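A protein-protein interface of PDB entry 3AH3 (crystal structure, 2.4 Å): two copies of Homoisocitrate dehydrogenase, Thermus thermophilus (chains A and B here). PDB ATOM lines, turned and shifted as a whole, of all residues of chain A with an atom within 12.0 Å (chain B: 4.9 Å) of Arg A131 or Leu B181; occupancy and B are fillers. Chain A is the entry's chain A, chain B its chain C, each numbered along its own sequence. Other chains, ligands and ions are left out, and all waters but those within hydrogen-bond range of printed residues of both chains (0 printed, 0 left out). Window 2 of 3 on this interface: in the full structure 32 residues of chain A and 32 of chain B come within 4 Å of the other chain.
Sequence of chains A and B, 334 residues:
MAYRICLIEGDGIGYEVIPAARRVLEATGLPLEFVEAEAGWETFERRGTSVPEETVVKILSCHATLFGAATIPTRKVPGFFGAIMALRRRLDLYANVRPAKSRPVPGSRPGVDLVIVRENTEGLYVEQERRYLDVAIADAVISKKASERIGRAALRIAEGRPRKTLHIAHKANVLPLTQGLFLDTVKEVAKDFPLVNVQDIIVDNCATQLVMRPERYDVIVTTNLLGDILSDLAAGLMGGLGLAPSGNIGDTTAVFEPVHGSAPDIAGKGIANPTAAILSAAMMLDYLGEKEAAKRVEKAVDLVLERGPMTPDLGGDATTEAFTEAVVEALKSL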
ATOM      1  N   GLU A 127      32.504  -1.418  28.144  1.00  0.00           N
ATOM      2  CA  GLU A 127      32.273  -0.892  26.797  1.00  0.00           C
ATOM      3  C   GLU A 127      30.910  -1.363  26.322  1.00  0.00           C
ATOM      4  O   GLU A 127      30.682  -2.560  26.148  1.00  0.00           O
ATOM      5  CB  GLU A 127      33.370  -1.321  25.823  1.00  0.00           C
ATOM      6  CG  GLU A 127      34.724  -0.675  26.092  1.00  0.00           C
ATOM      7  CD  GLU A 127      35.798  -1.176  25.151  1.00  0.00           C
ATOM      8  OE1 GLU A 127      35.850  -0.715  23.990  1.00  0.00           O
ATOM      9  OE2 GLU A 127      36.589  -2.043  25.573  1.00  0.00           O
ATOM     10  N   GLN A 128      30.013  -0.405  26.116  1.00  0.00           N
ATOM     11  CA  GLN A 128      28.593  -0.684  26.016  1.00  0.00           C
ATOM     12  C   GLN A 128      28.092  -0.990  24.598  1.00  0.00           C
ATOM     13  O   GLN A 128      28.629  -0.484  23.606  1.00  0.00           O
ATOM     14  CB  GLN A 128      27.823   0.491  26.605  1.00  0.00           C
ATOM     15  CG  GLN A 128      26.701   0.076  27.533  1.00  0.00           C
ATOM     16  CD  GLN A 128      27.203  -0.587  28.801  1.00  0.00           C
ATOM     17  OE1 GLN A 128      27.133  -1.806  28.937  1.00  0.00           O
ATOM     18  NE2 GLN A 128      27.725   0.213  29.728  1.00  0.00           N
ATOM     19  N   GLU A 129      27.063  -1.832  24.527  1.00  0.00           N
ATOM     20  CA  GLU A 129      26.353  -2.144  23.287  1.00  0.00           C
ATOM     21  C   GLU A 129      24.939  -1.615  23.368  1.00  0.00           C
ATOM     22  O   GLU A 129      24.322  -1.650  24.427  1.00  0.00           O
ATOM     23  CB  GLU A 129      26.257  -3.654  23.080  1.00  0.00           C
ATOM     24  CG  GLU A 129      27.460  -4.317  22.487  1.00  0.00           C
ATOM     25  CD  GLU A 129      27.147  -5.708  21.953  1.00  0.00           C
ATOM     26  OE1 GLU A 129      27.383  -5.937  20.751  1.00  0.00           O
ATOM     27  OE2 GLU A 129      26.655  -6.569  22.721  1.00  0.00           O
ATOM     28  N   ARG A 130      24.417  -1.144  22.242  1.00  0.00           N
ATOM     29  CA  ARG A 130      23.002  -0.782  22.143  1.00  0.00           C
ATOM     30  C   ARG A 130      22.379  -1.420  20.920  1.00  0.00           C
ATOM     31  O   ARG A 130      23.050  -1.644  19.907  1.00  0.00           O
ATOM     32  CB  ARG A 130      22.800   0.733  22.045  1.00  0.00           C
ATOM     33  CG  ARG A 130      23.191   1.508  23.277  1.00  0.00           C
ATOM     34  CD  ARG A 130      24.553   2.135  23.092  1.00  0.00           C
ATOM     35  NE  ARG A 130      24.466   3.282  22.194  1.00  0.00           N
ATOM     36  CZ  ARG A 130      25.489   3.772  21.498  1.00  0.00           C
ATOM     37  NH1 ARG A 130      25.300   4.826  20.710  1.00  0.00           N
ATOM     38  NH2 ARG A 130      26.691   3.206  21.580  1.00  0.00           N
ATOM     39  N   ARG A 131      21.092  -1.716  21.025  1.00  0.00           N
ATOM     40  CA  ARG A 131      20.304  -2.013  19.856  1.00  0.00           C
ATOM     41  C   ARG A 131      19.095  -1.107  19.819  1.00  0.00           C
ATOM     42  O   ARG A 131      18.347  -1.014  20.792  1.00  0.00           O
ATOM     43  CB  ARG A 131      19.891  -3.480  19.794  1.00  0.00           C
ATOM     44  CG  ARG A 131      19.133  -3.781  18.523  1.00  0.00           C
ATOM     45  CD  ARG A 131      19.156  -5.229  18.128  1.00  0.00           C
ATOM     46  NE  ARG A 131      18.184  -5.435  17.064  1.00  0.00           N
ATOM     47  CZ  ARG A 131      17.775  -6.619  16.630  1.00  0.00           C
ATOM     48  NH1 ARG A 131      18.256  -7.736  17.165  1.00  0.00           N
ATOM     49  NH2 ARG A 131      16.877  -6.682  15.660  1.00  0.00           N
ATOM     50  N   TYR A 132      18.939  -0.425  18.689  1.00  0.00           N
ATOM     51  CA  TYR A 132      17.785   0.424  18.437  1.00  0.00           C
ATOM     52  C   TYR A 132      17.083  -0.087  17.190  1.00  0.00           C
ATOM     53  O   TYR A 132      17.512   0.187  16.061  1.00  0.00           O
ATOM     54  CB  TYR A 132      18.204   1.889  18.258  1.00  0.00           C
ATOM     55  CG  TYR A 132      18.905   2.506  19.454  1.00  0.00           C
ATOM     56  CD1 TYR A 132      20.145   3.133  19.315  1.00  0.00           C
ATOM     57  CD2 TYR A 132      18.322   2.477  20.719  1.00  0.00           C
ATOM     58  CE1 TYR A 132      20.778   3.711  20.407  1.00  0.00           C
ATOM     59  CE2 TYR A 132      18.951   3.043  21.814  1.00  0.00           C
ATOM     60  CZ  TYR A 132      20.171   3.656  21.658  1.00  0.00           C
ATOM     61  OH  TYR A 132      20.778   4.222  22.757  1.00  0.00           O
ATOM     62  N   LEU A 133      16.003  -0.830  17.409  1.00  0.00           N
ATOM     63  CA  LEU A 133      15.263  -1.513  16.339  1.00  0.00           C
ATOM     64  C   LEU A 133      16.188  -2.469  15.578  1.00  0.00           C
ATOM     65  O   LEU A 133      16.745  -3.387  16.174  1.00  0.00           O
ATOM     66  CB  LEU A 133      14.564  -0.513  15.408  1.00  0.00           C
ATOM     67  CG  LEU A 133      13.464   0.387  15.988  1.00  0.00           C
ATOM     68  CD1 LEU A 133      12.970   1.349  14.935  1.00  0.00           C
ATOM     69  CD2 LEU A 133      12.287  -0.417  16.543  1.00  0.00           C
ATOM     70  N   ASP A 134      16.369  -2.235  14.280  1.00  0.00           N
ATOM     71  CA  ASP A 134      17.211  -3.142  13.499  1.00  0.00           C
ATOM     72  C   ASP A 134      18.650  -2.637  13.332  1.00  0.00           C
ATOM     73  O   ASP A 134      19.418  -3.163  12.523  1.00  0.00           O
ATOM     74  CB  ASP A 134      16.551  -3.513  12.166  1.00  0.00           C
ATOM     75  CG  ASP A 134      15.484  -4.591  12.322  1.00  0.00           C
ATOM     76  OD1 ASP A 134      14.819  -4.917  11.313  1.00  0.00           O
ATOM     77  OD2 ASP A 134      15.309  -5.114  13.449  1.00  0.00           O
ATOM     78  N   VAL A 135      19.029  -1.656  14.155  1.00  0.00           N
ATOM     79  CA  VAL A 135      20.395  -1.127  14.165  1.00  0.00           C
ATOM     80  C   VAL A 135      21.068  -1.356  15.515  1.00  0.00           C
ATOM     81  O   VAL A 135      20.616  -0.841  16.544  1.00  0.00           O
ATOM     82  CB  VAL A 135      20.442   0.392  13.842  1.00  0.00           C
ATOM     83  CG1 VAL A 135      21.886   0.904  13.886  1.00  0.00           C
ATOM     84  CG2 VAL A 135      19.812   0.687  12.486  1.00  0.00           C
ATOM     85  N   ALA A 136      22.164  -2.108  15.490  1.00  0.00           N
ATOM     86  CA  ALA A 136      22.957  -2.385  16.675  1.00  0.00           C
ATOM     87  C   ALA A 136      24.314  -1.674  16.616  1.00  0.00           C
ATOM     88  O   ALA A 136      24.973  -1.646  15.572  1.00  0.00           O
ATOM     89  CB  ALA A 136      23.134  -3.881  16.841  1.00  0.00           C
ATOM     90  N   ILE A 137      24.713  -1.084  17.739  1.00  0.00           N
ATOM     91  CA  ILE A 137      25.976  -0.347  17.830  1.00  0.00           C
ATOM     92  C   ILE A 137      26.770  -0.774  19.062  1.00  0.00           C
ATOM     93  O   ILE A 137      26.260  -0.732  20.194  1.00  0.00           O
ATOM     94  CB  ILE A 137      25.739   1.182  17.896  1.00  0.00           C
ATOM     95  CG1 ILE A 137      24.792   1.633  16.784  1.00  0.00           C
ATOM     96  CG2 ILE A 137      27.056   1.938  17.804  1.00  0.00           C
ATOM     97  CD1 ILE A 137      23.832   2.656  17.231  1.00  0.00           C
ATOM     98  N   ALA A 138      28.007  -1.199  18.843  1.00  0.00           N
ATOM     99  CA  ALA A 138      28.925  -1.459  19.947  1.00  0.00           C
ATOM    100  C   ALA A 138      29.965  -0.349  20.011  1.00  0.00           C
ATOM    101  O   ALA A 138      30.569  -0.005  18.998  1.00  0.00           O
ATOM    102  CB  ALA A 138      29.592  -2.814  19.789  1.00  0.00           C
ATOM    103  N   ASP A 139      30.154   0.219  21.201  1.00  0.00           N
ATOM    104  CA  ASP A 139      31.208   1.210  21.435  1.00  0.00           C
ATOM    105  C   ASP A 139      32.605   0.579  21.500  1.00  0.00           C
ATOM    106  O   ASP A 139      32.834  -0.387  22.242  1.00  0.00           O
ATOM    107  CB  ASP A 139      30.943   1.965  22.740  1.00  0.00           C
ATOM    108  CG  ASP A 139      29.875   3.058  22.605  1.00  0.00           C
ATOM    109  OD1 ASP A 139      29.227   3.190  21.545  1.00  0.00           O
ATOM    110  OD2 ASP A 139      29.691   3.806  23.586  1.00  0.00           O
ATOM    111  N   ILE B 142      26.187  -2.753  13.186  1.00  0.00           N
ATOM    112  CA  ILE B 142      25.556  -3.857  12.480  1.00  0.00           C
ATOM    113  C   ILE B 142      24.054  -3.571  12.293  1.00  0.00           C
ATOM    114  O   ILE B 142      23.355  -3.270  13.254  1.00  0.00           O
ATOM    115  CB  ILE B 142      25.733  -5.173  13.271  1.00  0.00           C
ATOM    116  CG1 ILE B 142      27.226  -5.565  13.408  1.00  0.00           C
ATOM    117  CG2 ILE B 142      24.886  -6.298  12.677  1.00  0.00           C
ATOM    118  CD1 ILE B 142      27.960  -5.850  12.096  1.00  0.00           C
ATOM    119  N   SER B 143      23.561  -3.642  11.058  1.00  0.00           N
ATOM    120  CA  SER B 143      22.114  -3.643  10.841  1.00  0.00           C
ATOM    121  C   SER B 143      21.636  -4.953  10.230  1.00  0.00           C
ATOM    122  O   SER B 143      22.416  -5.686   9.617  1.00  0.00           O
ATOM    123  CB  SER B 143      21.655  -2.450  10.000  1.00  0.00           C
ATOM    124  OG  SER B 143      22.238  -2.473   8.719  1.00  0.00           O
ATOM    125  N   LYS B 144      20.351  -5.245  10.427  1.00  0.00           N
ATOM    126  CA  LYS B 144      19.719  -6.440   9.872  1.00  0.00           C
ATOM    127  C   LYS B 144      19.766  -6.430   8.360  1.00  0.00           C
ATOM    128  O   LYS B 144      20.126  -7.434   7.738  1.00  0.00           O
ATOM    129  CB  LYS B 144      18.270  -6.537  10.320  1.00  0.00           C
ATOM    130  CG  LYS B 144      17.687  -7.918  10.173  1.00  0.00           C
ATOM    131  CD  LYS B 144      16.422  -8.017  10.991  1.00  0.00           C
ATOM    132  CE  LYS B 144      16.328  -9.361  11.673  1.00  0.00           C
ATOM    133  NZ  LYS B 144      15.281  -9.288  12.736  1.00  0.00           N
ATOM    134  N   SER B 147      23.194  -7.089   7.147  1.00  0.00           N
ATOM    135  CA  SER B 147      23.610  -8.457   7.411  1.00  0.00           C
ATOM    136  C   SER B 147      22.905  -9.445   6.486  1.00  0.00           C
ATOM    137  O   SER B 147      23.502 -10.444   6.086  1.00  0.00           O
ATOM    138  CB  SER B 147      23.376  -8.840   8.874  1.00  0.00           C
ATOM    139  OG  SER B 147      24.111  -8.011   9.742  1.00  0.00           O
ATOM    140  N   PRO B 176      27.112  -9.855  22.055  1.00  0.00           N
ATOM    141  CA  PRO B 176      25.837 -10.544  21.802  1.00  0.00           C
ATOM    142  C   PRO B 176      24.779  -9.720  21.066  1.00  0.00           C
ATOM    143  O   PRO B 176      23.934 -10.301  20.379  1.00  0.00           O
ATOM    144  CB  PRO B 176      25.340 -10.898  23.209  1.00  0.00           C
ATOM    145  CG  PRO B 176      26.032  -9.947  24.114  1.00  0.00           C
ATOM    146  CD  PRO B 176      27.376  -9.732  23.502  1.00  0.00           C
ATOM    147  N   LEU B 177      24.814  -8.394  21.211  1.00  0.00           N
ATOM    148  CA  LEU B 177      23.867  -7.533  20.500  1.00  0.00           C
ATOM    149  C   LEU B 177      24.294  -7.248  19.055  1.00  0.00           C
ATOM    150  O   LEU B 177      23.484  -7.403  18.144  1.00  0.00           O
ATOM    151  CB  LEU B 177      23.557  -6.233  21.271  1.00  0.00           C
ATOM    152  CG  LEU B 177      22.894  -6.364  22.658  1.00  0.00           C
ATOM    153  CD1 LEU B 177      22.583  -4.996  23.261  1.00  0.00           C
ATOM    154  CD2 LEU B 177      21.634  -7.223  22.632  1.00  0.00           C
ATOM    155  N   THR B 178      25.541  -6.845  18.829  1.00  0.00           N
ATOM    156  CA  THR B 178      25.966  -6.514  17.453  1.00  0.00           C
ATOM    157  C   THR B 178      26.333  -7.756  16.650  1.00  0.00           C
ATOM    158  O   THR B 178      25.680  -8.080  15.659  1.00  0.00           O
ATOM    159  CB  THR B 178      27.098  -5.452  17.388  1.00  0.00           C
ATOM    160  OG1 THR B 178      28.262  -5.919  18.086  1.00  0.00           O
ATOM    161  CG2 THR B 178      26.633  -4.139  17.996  1.00  0.00           C
ATOM    162  N   GLN B 179      27.352  -8.472  17.099  1.00  0.00           N
ATOM    163  CA  GLN B 179      27.767  -9.703  16.426  1.00  0.00           C
ATOM    164  C   GLN B 179      26.692 -10.796  16.468  1.00  0.00           C
ATOM    165  O   GLN B 179      26.615 -11.623  15.572  1.00  0.00           O
ATOM    166  CB  GLN B 179      29.100 -10.205  16.997  1.00  0.00           C
ATOM    167  CG  GLN B 179      30.282  -9.276  16.741  1.00  0.00           C
ATOM    168  CD  GLN B 179      30.832  -9.413  15.343  1.00  0.00           C
ATOM    169  OE1 GLN B 179      31.005 -10.521  14.850  1.00  0.00           O
ATOM    170  NE2 GLN B 179      31.125  -8.290  14.696  1.00  0.00           N
ATOM    171  N   GLY B 180      25.854 -10.786  17.498  1.00  0.00           N
ATOM    172  CA  GLY B 180      24.761 -11.750  17.599  1.00  0.00           C
ATOM    173  C   GLY B 180      23.692 -11.493  16.558  1.00  0.00           C
ATOM    174  O   GLY B 180      23.107 -12.426  16.020  1.00  0.00           O
ATOM    175  N   LEU B 181      23.444 -10.218  16.274  1.00  0.00           N
ATOM    176  CA  LEU B 181      22.495  -9.817  15.242  1.00  0.00           C
ATOM    177  C   LEU B 181      23.004 -10.236  13.854  1.00  0.00           C
ATOM    178  O   LEU B 181      22.232 -10.689  13.000  1.00  0.00           O
ATOM    179  CB  LEU B 181      22.258  -8.305  15.326  1.00  0.00           C
ATOM    180  CG  LEU B 181      21.073  -7.585  14.664  1.00  0.00           C
ATOM    181  CD1 LEU B 181      21.540  -6.754  13.482  1.00  0.00           C
ATOM    182  CD2 LEU B 181      19.877  -8.500  14.283  1.00  0.00           C
ATOM    183  N   PHE B 182      24.307 -10.101  13.644  1.00  0.00           N
ATOM    184  CA  PHE B 182      24.926 -10.529  12.396  1.00  0.00           C
ATOM    185  C   PHE B 182      24.865 -12.057  12.230  1.00  0.00           C
ATOM    186  O   PHE B 182      24.458 -12.547  11.170  1.00  0.00           O
ATOM    187  CB  PHE B 182      26.366 -10.029  12.324  1.00  0.00           C
ATOM    188  CG  PHE B 182      27.153 -10.599  11.179  1.00  0.00           C
ATOM    189  CD1 PHE B 182      27.020 -10.074   9.897  1.00  0.00           C
ATOM    190  CD2 PHE B 182      28.058 -11.646  11.393  1.00  0.00           C
ATOM    191  CE1 PHE B 182      27.752 -10.595   8.850  1.00  0.00           C
ATOM    192  CE2 PHE B 182      28.793 -12.161  10.361  1.00  0.00           C
ATOM    193  CZ  PHE B 182      28.639 -11.644   9.082  1.00  0.00           C
ATOM    194  N   LEU B 183      25.255 -12.790  13.281  1.00  0.00           N
ATOM    195  CA  LEU B 183      25.211 -14.253  13.281  1.00  0.00           C
ATOM    196  C   LEU B 183      23.823 -14.745  12.887  1.00  0.00           C
ATOM    197  O   LEU B 183      23.671 -15.454  11.886  1.00  0.00           O
ATOM    198  CB  LEU B 183      25.578 -14.820  14.662  1.00  0.00           C
ATOM    199  CG  LEU B 183      26.300 -16.177  14.794  1.00  0.00           C
ATOM    200  CD1 LEU B 183      25.930 -16.882  16.089  1.00  0.00           C
ATOM    201  CD2 LEU B 183      26.101 -17.121  13.633  1.00  0.00           C
ATOM    202  N   ASP B 184      22.826 -14.346  13.678  1.00  0.00           N
ATOM    203  CA  ASP B 184      21.438 -14.782  13.536  1.00  0.00           C
ATOM    204  C   ASP B 184      20.851 -14.506  12.163  1.00  0.00           C
ATOM    205  O   ASP B 184      20.195 -15.360  11.588  1.00  0.00           O
ATOM    206  CB  ASP B 184      20.554 -14.113  14.595  1.00  0.00           C
ATOM    207  CG  ASP B 184      20.798 -14.648  15.994  1.00  0.00           C
ATOM    208  OD1 ASP B 184      21.269 -15.800  16.132  1.00  0.00           O
ATOM    209  OD2 ASP B 184      20.515 -13.912  16.967  1.00  0.00           O
ATOM    210  N   THR B 185      21.100 -13.312  11.644  1.00  0.00           N
ATOM    211  CA  THR B 185      20.522 -12.891  10.387  1.00  0.00           C
ATOM    212  C   THR B 185      21.082 -13.696   9.210  1.00  0.00           C
ATOM    213  O   THR B 185      20.322 -14.129   8.342  1.00  0.00           O
ATOM    214  CB  THR B 185      20.707 -11.385  10.181  1.00  0.00           C
ATOM    215  OG1 THR B 185      20.289 -10.700  11.367  1.00  0.00           O
ATOM    216  CG2 THR B 185      19.888 -10.897   8.996  1.00  0.00           C
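The side-chain carboxylate (OE2) of Glu A129 sits at hydrogen-bond distance from the backbone NH (N) of Leu B177 (3.0 Å).
The side-chain hydroxyl of Thr B178 sits at hydrogen-bond distance from the side-chain carboxylate of Glu A129 (2.8 Å).
The backbone carbonyl oxygen (O) of Asp A134 is in hydrogen-bond range of the backbone NH (N) of Lys B144 (3.1 Å).
The backbone carbonyl oxygen (O) of Ile B142 is in hydrogen-bond range of the backbone NH (N) of Ala A136, 2.8 Å away.
The side-chain carboxylate (OE2) of Glu A129 lies close to the backbone nitrogen (N) of Pro B176 (3.4 Å).
Hydrophobic or aromatic side chains of chain A within 4 Å of the printed part of chain B: Ala A136 and Ala A138.
Along chain A the printed residues that touch a printed residue of chain B span positions 129 to 138.
Among the printed residues, 12 pairs touch across the chains.
Among the printed residues, no Asp or Glu carboxylate lies within 4 Å of a Lys or Arg side-chain nitrogen of the other chain.
The backbone NH (N) of Arg A130 sits at hydrogen-bond distance from the backbone carbonyl oxygen (O) of Ile A137.
The guanidinium group (NE) of Arg A131 sits at hydrogen-bond distance from the backbone carbonyl oxygen (O) of Leu A133 (2.7 Å).
The side-chain carboxylate of Asp A134 is in salt-bridge range of the guanidinium group of Arg A131, 3.1 Å away.
The backbone carbonyl oxygen (O) of Ser B143 sits at hydrogen-bond distance from the side-chain hydroxyl (OG) of Ser B147.
O of Leu B181 is in hydrogen-bond range of OG1 of Thr B185 (2.5 Å).
No position is printed for both chains.
Of the 12 pairs that touch across the chains among the printed residues, none has its exchanged pair printed and touching as well.
Among the printed residues, merely in contact across the chains: Asp A134 with Ser B143 (3.2 Å), Ala A138 with Thr B178 (3.4 Å), Arg A131 with Leu B181 (3.4 Å), Ile A137 with Thr B178 (3.5 Å), Ala A136 with Thr B178 (3.7 Å), Val A135 with Ile B142 (3.7 Å) and Ala A136 with Leu B177 (3.8 Å).
Of the printed residues of chain B, Glu A129 touches Pro B176 (3.3 Å), Leu B177 (3.0 Å) and Thr B178 (2.8 Å).
Arg A130 touches none of the printed residues of chain B.
Printed residues of chain B within 4 Å of Ala A136: Ile B142 (2.8 Å), Leu B177 (3.8 Å) and Thr B178 (3.7 Å).
Asp A139 touches none of the printed residues of chain B.
Of the printed residues of chain A, Ser B143 touches Asp A134.
Of chain A, only Glu A129 and Ala A136 come within 4 Å of Leu B177.
Thr B178 touches just these residues of chain A: Glu A129 (2.8 Å), Ala A136 (3.7 Å), Ile A137 (3.5 Å) and Ala A138 (3.4 Å).
Gly B180 touches none of the printed residues of chain A.
Of chain A, only Arg A131 (3.4 Å) comes within 4 Å of Leu B181.
No residue of chain A comes within 4 Å of Phe B182.
No residue of chain A comes within 4 Å of Leu B183.
No residue of chain A comes within 4 Å of Asp B184.
No residue of chain A comes within 4 Å of Thr B185.
The nearest printed residue of chain B that does not touch Arg A131 is Lys B144 (4.2 Å).
The nearest printed residue of chain B that does not touch Ile A137 is Ile B142 (5.1 Å).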
